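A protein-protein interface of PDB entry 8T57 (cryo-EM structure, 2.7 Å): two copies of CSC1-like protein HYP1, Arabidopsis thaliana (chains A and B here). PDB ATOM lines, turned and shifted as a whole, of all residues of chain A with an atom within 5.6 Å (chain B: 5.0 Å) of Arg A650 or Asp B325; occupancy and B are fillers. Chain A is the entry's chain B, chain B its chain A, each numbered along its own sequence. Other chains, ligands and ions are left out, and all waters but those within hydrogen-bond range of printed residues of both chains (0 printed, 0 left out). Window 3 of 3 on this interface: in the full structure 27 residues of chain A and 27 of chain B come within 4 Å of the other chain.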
ATOM      1  N   LEU A 172     -17.241  16.202   5.627  1.00  0.00           N
ATOM      2  CA  LEU A 172     -17.508  14.801   5.494  1.00  0.00           C
ATOM      3  C   LEU A 172     -17.497  14.347   4.067  1.00  0.00           C
ATOM      4  O   LEU A 172     -16.948  13.291   3.785  1.00  0.00           O
ATOM      5  CB  LEU A 172     -18.803  14.406   6.130  1.00  0.00           C
ATOM      6  CG  LEU A 172     -18.826  14.395   7.613  1.00  0.00           C
ATOM      7  CD1 LEU A 172     -20.191  14.213   8.031  1.00  0.00           C
ATOM      8  CD2 LEU A 172     -17.986  13.239   8.149  1.00  0.00           C
ATOM      9  N   ILE A 645     -26.156  19.079  19.292  1.00  0.00           N
ATOM     10  CA  ILE A 645     -26.487  17.686  19.510  1.00  0.00           C
ATOM     11  C   ILE A 645     -26.899  17.054  18.215  1.00  0.00           C
ATOM     12  O   ILE A 645     -26.494  15.932  17.918  1.00  0.00           O
ATOM     13  CB  ILE A 645     -27.536  17.468  20.582  1.00  0.00           C
ATOM     14  CG1 ILE A 645     -26.926  17.853  21.922  1.00  0.00           C
ATOM     15  CG2 ILE A 645     -27.965  15.992  20.566  1.00  0.00           C
ATOM     16  CD1 ILE A 645     -27.898  17.974  23.056  1.00  0.00           C
ATOM     17  N   TYR A 646     -27.693  17.740  17.429  1.00  0.00           N
ATOM     18  CA  TYR A 646     -28.067  17.210  16.154  1.00  0.00           C
ATOM     19  C   TYR A 646     -26.814  16.848  15.381  1.00  0.00           C
ATOM     20  O   TYR A 646     -26.725  15.735  14.882  1.00  0.00           O
ATOM     21  CB  TYR A 646     -28.913  18.203  15.380  1.00  0.00           C
ATOM     22  CG  TYR A 646     -29.194  17.772  14.034  1.00  0.00           C
ATOM     23  CD1 TYR A 646     -30.178  16.883  13.802  1.00  0.00           C
ATOM     24  CD2 TYR A 646     -28.443  18.260  13.013  1.00  0.00           C
ATOM     25  CE1 TYR A 646     -30.420  16.469  12.539  1.00  0.00           C
ATOM     26  CE2 TYR A 646     -28.680  17.849  11.762  1.00  0.00           C
ATOM     27  CZ  TYR A 646     -29.663  16.957  11.517  1.00  0.00           C
ATOM     28  OH  TYR A 646     -29.894  16.528  10.242  1.00  0.00           O
ATOM     29  N   CYS A 647     -25.833  17.762  15.310  1.00  0.00           N
ATOM     30  CA  CYS A 647     -24.571  17.531  14.609  1.00  0.00           C
ATOM     31  C   CYS A 647     -23.747  16.417  15.255  1.00  0.00           C
ATOM     32  O   CYS A 647     -23.090  15.637  14.558  1.00  0.00           O
ATOM     33  CB  CYS A 647     -23.745  18.805  14.567  1.00  0.00           C
ATOM     34  SG  CYS A 647     -24.446  20.071  13.538  1.00  0.00           S
ATOM     35  N   GLN A 648     -23.840  16.280  16.572  1.00  0.00           N
ATOM     36  CA  GLN A 648     -23.157  15.224  17.296  1.00  0.00           C
ATOM     37  C   GLN A 648     -23.712  13.880  16.928  1.00  0.00           C
ATOM     38  O   GLN A 648     -23.020  12.874  17.018  1.00  0.00           O
ATOM     39  CB  GLN A 648     -23.270  15.393  18.793  1.00  0.00           C
ATOM     40  CG  GLN A 648     -22.512  16.532  19.375  1.00  0.00           C
ATOM     41  CD  GLN A 648     -22.916  16.746  20.763  1.00  0.00           C
ATOM     42  OE1 GLN A 648     -23.221  15.771  21.448  1.00  0.00           O
ATOM     43  NE2 GLN A 648     -22.972  17.989  21.203  1.00  0.00           N
ATOM     44  N   ARG A 649     -24.980  13.819  16.582  1.00  0.00           N
ATOM     45  CA  ARG A 649     -25.539  12.561  16.168  1.00  0.00           C
ATOM     46  C   ARG A 649     -25.484  12.381  14.654  1.00  0.00           C
ATOM     47  O   ARG A 649     -25.335  11.265  14.175  1.00  0.00           O
ATOM     48  CB  ARG A 649     -26.963  12.457  16.648  1.00  0.00           C
ATOM     49  CG  ARG A 649     -27.100  12.366  18.159  1.00  0.00           C
ATOM     50  CD  ARG A 649     -28.500  12.285  18.565  1.00  0.00           C
ATOM     51  NE  ARG A 649     -28.661  12.219  20.018  1.00  0.00           N
ATOM     52  CZ  ARG A 649     -29.862  12.163  20.643  1.00  0.00           C
ATOM     53  NH1 ARG A 649     -30.978  12.151  19.933  1.00  0.00           N
ATOM     54  NH2 ARG A 649     -29.930  12.121  21.964  1.00  0.00           N
ATOM     55  N   ARG A 650     -25.592  13.476  13.907  1.00  0.00           N
ATOM     56  CA  ARG A 650     -25.677  13.485  12.455  1.00  0.00           C
ATOM     57  C   ARG A 650     -24.368  13.465  11.687  1.00  0.00           C
ATOM     58  O   ARG A 650     -24.316  12.931  10.581  1.00  0.00           O
ATOM     59  CB  ARG A 650     -26.468  14.705  12.004  1.00  0.00           C
ATOM     60  CG  ARG A 650     -26.602  14.914  10.510  1.00  0.00           C
ATOM     61  CD  ARG A 650     -27.358  13.859   9.869  1.00  0.00           C
ATOM     62  NE  ARG A 650     -27.454  14.033   8.452  1.00  0.00           N
ATOM     63  CZ  ARG A 650     -26.501  13.705   7.560  1.00  0.00           C
ATOM     64  NH1 ARG A 650     -25.342  13.232   7.954  1.00  0.00           N
ATOM     65  NH2 ARG A 650     -26.742  13.860   6.273  1.00  0.00           N
ATOM     66  N   PHE A 651     -23.335  14.119  12.199  1.00  0.00           N
ATOM     67  CA  PHE A 651     -22.093  14.229  11.466  1.00  0.00           C
ATOM     68  C   PHE A 651     -20.899  13.711  12.223  1.00  0.00           C
ATOM     69  O   PHE A 651     -20.097  12.949  11.688  1.00  0.00           O
ATOM     70  CB  PHE A 651     -21.803  15.689  11.160  1.00  0.00           C
ATOM     71  CG  PHE A 651     -22.824  16.401  10.361  1.00  0.00           C
ATOM     72  CD1 PHE A 651     -23.476  17.455  10.900  1.00  0.00           C
ATOM     73  CD2 PHE A 651     -23.131  16.040   9.097  1.00  0.00           C
ATOM     74  CE1 PHE A 651     -24.400  18.142  10.194  1.00  0.00           C
ATOM     75  CE2 PHE A 651     -24.047  16.719   8.386  1.00  0.00           C
ATOM     76  CZ  PHE A 651     -24.680  17.773   8.931  1.00  0.00           C
ATOM     77  N   LEU A 652     -20.785  14.074  13.491  1.00  0.00           N
ATOM     78  CA  LEU A 652     -19.552  13.796  14.199  1.00  0.00           C
ATOM     79  C   LEU A 652     -19.106  12.347  14.316  1.00  0.00           C
ATOM     80  O   LEU A 652     -17.905  12.112  14.272  1.00  0.00           O
ATOM     81  CB  LEU A 652     -19.496  14.473  15.556  1.00  0.00           C
ATOM     82  CG  LEU A 652     -19.372  16.036  15.528  1.00  0.00           C
ATOM     83  CD1 LEU A 652     -19.430  16.563  16.921  1.00  0.00           C
ATOM     84  CD2 LEU A 652     -18.066  16.482  14.906  1.00  0.00           C
ATOM     85  N   PRO A 653     -19.952  11.332  14.456  1.00  0.00           N
ATOM     86  CA  PRO A 653     -19.522   9.964  14.552  1.00  0.00           C
ATOM     87  C   PRO A 653     -18.695   9.534  13.351  1.00  0.00           C
ATOM     88  O   PRO A 653     -17.853   8.639  13.468  1.00  0.00           O
ATOM     89  CB  PRO A 653     -20.840   9.216  14.616  1.00  0.00           C
ATOM     90  CG  PRO A 653     -21.797  10.214  15.175  1.00  0.00           C
ATOM     91  CD  PRO A 653     -21.371  11.508  14.588  1.00  0.00           C
ATOM     92  N   ASN A 654     -18.839  10.214  12.210  1.00  0.00           N
ATOM     93  CA  ASN A 654     -18.105   9.792  11.040  1.00  0.00           C
ATOM     94  C   ASN A 654     -16.670  10.251  11.062  1.00  0.00           C
ATOM     95  O   ASN A 654     -15.891   9.879  10.185  1.00  0.00           O
ATOM     96  CB  ASN A 654     -18.784  10.229   9.780  1.00  0.00           C
ATOM     97  CG  ASN A 654     -20.001   9.469   9.469  1.00  0.00           C
ATOM     98  OD1 ASN A 654     -20.253   8.379   9.968  1.00  0.00           O
ATOM     99  ND2 ASN A 654     -20.777  10.003   8.587  1.00  0.00           N
ATOM    100  N   GLN A 661     -21.572   0.745   5.714  1.00  0.00           N
ATOM    101  CA  GLN A 661     -21.794   0.940   4.296  1.00  0.00           C
ATOM    102  C   GLN A 661     -20.538   1.425   3.590  1.00  0.00           C
ATOM    103  O   GLN A 661     -20.143   0.893   2.554  1.00  0.00           O
ATOM    104  CB  GLN A 661     -22.943   1.927   4.135  1.00  0.00           C
ATOM    105  CG  GLN A 661     -23.324   2.269   2.759  1.00  0.00           C
ATOM    106  CD  GLN A 661     -24.568   3.133   2.705  1.00  0.00           C
ATOM    107  OE1 GLN A 661     -24.887   3.978   3.579  1.00  0.00           O
ATOM    108  NE2 GLN A 661     -25.324   2.919   1.644  1.00  0.00           N
ATOM    109  N   GLN B 321     -22.251   1.535  13.342  1.00  0.00           N
ATOM    110  CA  GLN B 321     -23.064   2.438  12.522  1.00  0.00           C
ATOM    111  C   GLN B 321     -23.191   1.844  11.155  1.00  0.00           C
ATOM    112  O   GLN B 321     -22.201   1.349  10.613  1.00  0.00           O
ATOM    113  CB  GLN B 321     -22.428   3.806  12.392  1.00  0.00           C
ATOM    114  CG  GLN B 321     -23.238   4.802  11.584  1.00  0.00           C
ATOM    115  CD  GLN B 321     -22.517   6.057  11.463  1.00  0.00           C
ATOM    116  OE1 GLN B 321     -21.928   6.511  12.437  1.00  0.00           O
ATOM    117  NE2 GLN B 321     -22.506   6.633  10.282  1.00  0.00           N
ATOM    118  N   GLY B 323     -25.360   3.129   8.040  1.00  0.00           N
ATOM    119  CA  GLY B 323     -25.308   3.904   6.814  1.00  0.00           C
ATOM    120  C   GLY B 323     -24.342   5.054   6.922  1.00  0.00           C
ATOM    121  O   GLY B 323     -23.859   5.348   8.015  1.00  0.00           O
ATOM    122  N   ILE B 324     -24.173   5.777   5.815  1.00  0.00           N
ATOM    123  CA  ILE B 324     -23.294   6.942   5.801  1.00  0.00           C
ATOM    124  C   ILE B 324     -23.887   7.974   6.721  1.00  0.00           C
ATOM    125  O   ILE B 324     -23.194   8.669   7.460  1.00  0.00           O
ATOM    126  CB  ILE B 324     -23.166   7.585   4.403  1.00  0.00           C
ATOM    127  CG1 ILE B 324     -22.573   6.592   3.356  1.00  0.00           C
ATOM    128  CG2 ILE B 324     -22.296   8.847   4.489  1.00  0.00           C
ATOM    129  CD1 ILE B 324     -21.219   5.999   3.649  1.00  0.00           C
ATOM    130  N   ASP B 325     -25.189   8.108   6.619  1.00  0.00           N
ATOM    131  CA  ASP B 325     -25.966   9.018   7.419  1.00  0.00           C
ATOM    132  C   ASP B 325     -26.457   8.305   8.663  1.00  0.00           C
ATOM    133  O   ASP B 325     -27.375   7.504   8.552  1.00  0.00           O
ATOM    134  CB  ASP B 325     -27.148   9.501   6.621  1.00  0.00           C
ATOM    135  CG  ASP B 325     -28.021  10.445   7.375  1.00  0.00           C
ATOM    136  OD1 ASP B 325     -27.873  10.569   8.584  1.00  0.00           O
ATOM    137  OD2 ASP B 325     -28.897  10.998   6.764  1.00  0.00           O
ATOM    138  N   PRO B 326     -25.938   8.592   9.853  1.00  0.00           N
ATOM    139  CA  PRO B 326     -26.197   7.904  11.092  1.00  0.00           C
ATOM    140  C   PRO B 326     -27.596   8.069  11.610  1.00  0.00           C
ATOM    141  O   PRO B 326     -27.969   7.412  12.574  1.00  0.00           O
ATOM    142  CB  PRO B 326     -25.209   8.549  12.046  1.00  0.00           C
ATOM    143  CG  PRO B 326     -24.983   9.867  11.494  1.00  0.00           C
ATOM    144  CD  PRO B 326     -25.051   9.719  10.014  1.00  0.00           C
ATOM    145  N   THR B 327     -28.371   8.974  11.020  1.00  0.00           N
ATOM    146  CA  THR B 327     -29.713   9.200  11.524  1.00  0.00           C
ATOM    147  C   THR B 327     -30.714   8.328  10.795  1.00  0.00           C
ATOM    148  O   THR B 327     -31.907   8.357  11.093  1.00  0.00           O
ATOM    149  CB  THR B 327     -30.115  10.676  11.455  1.00  0.00           C
ATOM    150  OG1 THR B 327     -30.177  11.131  10.097  1.00  0.00           O
ATOM    151  CG2 THR B 327     -29.110  11.519  12.223  1.00  0.00           C
ATOM    152  N   GLN B 328     -30.231   7.532   9.856  1.00  0.00           N
ATOM    153  CA  GLN B 328     -31.071   6.617   9.114  1.00  0.00           C
ATOM    154  C   GLN B 328     -30.401   5.258   9.124  1.00  0.00           C
ATOM    155  O   GLN B 328     -29.208   5.157   9.374  1.00  0.00           O
ATOM    156  CB  GLN B 328     -31.448   7.147   7.731  1.00  0.00           C
ATOM    157  CG  GLN B 328     -30.379   7.478   6.815  1.00  0.00           C
ATOM    158  CD  GLN B 328     -30.965   8.026   5.519  1.00  0.00           C
ATOM    159  OE1 GLN B 328     -31.786   7.368   4.890  1.00  0.00           O
ATOM    160  NE2 GLN B 328     -30.582   9.230   5.116  1.00  0.00           N
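Of the 12 printed residues of chain A, 5 touch a printed residue of chain B.
Printed residues of chain A that touch a printed residue of chain B: Arg A649, Arg A650, Pro A653, Asn A654 and Gln A661.
Hydrophobic or aromatic side chains of chain A that line the printed part of chain B: Pro A653.
Of the 7 printed residues of chain B, 6 touch a printed residue of chain A.
Printed residues of chain B that touch a printed residue of chain A: Gln B321, Gly B323, Ile B324, Asp B325, Pro B326 and Thr B327.
Hydrophobic or aromatic side chains of chain B within 4 Å of the printed part of chain A: Ile B324 and Pro B326.
Among the printed residues, Asp or Glu carboxylates within 4 Å of a Lys or Arg side-chain nitrogen of the other chain: Arg A650 with Asp B325.
NE2 of Gln B321 sits at hydrogen-bond distance from O of Gly B323 (2.9 Å).
The side-chain carboxylate of Asp B325 is in hydrogen-bond range of the side-chain hydroxyl of Thr B327 (2.8 Å).
OD2 of Asp B325 sits at hydrogen-bond distance from NE2 of Gln B328, at 2.9 Å.
Of chain B, only Asp B325 (3.5 Å), Pro B326 (3.3 Å) and Thr B327 (3.8 Å) come within 4 Å of Arg A650.
Of chain A, only Arg A650 comes within 4 Å of Asp B325.
Of the printed residues of chain A, Gly B323 touches Gln A661.
Printed residues of chain A within 4 Å of Pro B326: Arg A649 and Arg A650.
Of the printed residues of chain A, Ile B324 touches Asn A654 (3.0 Å) and Gln A661 (3.0 Å).
Of the printed residues of chain A, Gln B321 touches Pro A653 (3.6 Å) and Asn A654 (2.9 Å).
Printed residues of chain B within 4 Å of Asn A654: Gln B321 and Ile B324.
Ile A645 touches none of the printed residues of chain B.
The nearest printed residue of chain A that does not touch Gly B323 is Asn A654 (5.1 Å).
The side-chain amide nitrogen (NE2) of Gln B321 lies within hydrogen-bond range of the side-chain amide oxygen (OD1) of Asn A654 (2.9 Å).
The backbone carbonyl oxygen (O) of Ile B324 lies within hydrogen-bond range of the side-chain amide nitrogen (ND2) of Asn A654 (3.0 Å).
The backbone NH of Ile B324 lies within hydrogen-bond range of the side-chain amide oxygen of Gln A661.
The side-chain carboxylate (OD1) of Asp B325 is in salt-bridge range of the guanidinium group (NE) of Arg A650, at 3.5 Å.
Among the printed residues, merely in contact across the chains: Arg A649 with Pro B326 (3.0 Å), Gln A661 with Gly B323 (3.3 Å), Arg A650 with Pro B326 (3.3 Å), Pro A653 with Gln B321 (3.6 Å) and Arg A650 with Thr B327 (3.8 Å).
No position is printed for both chains.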
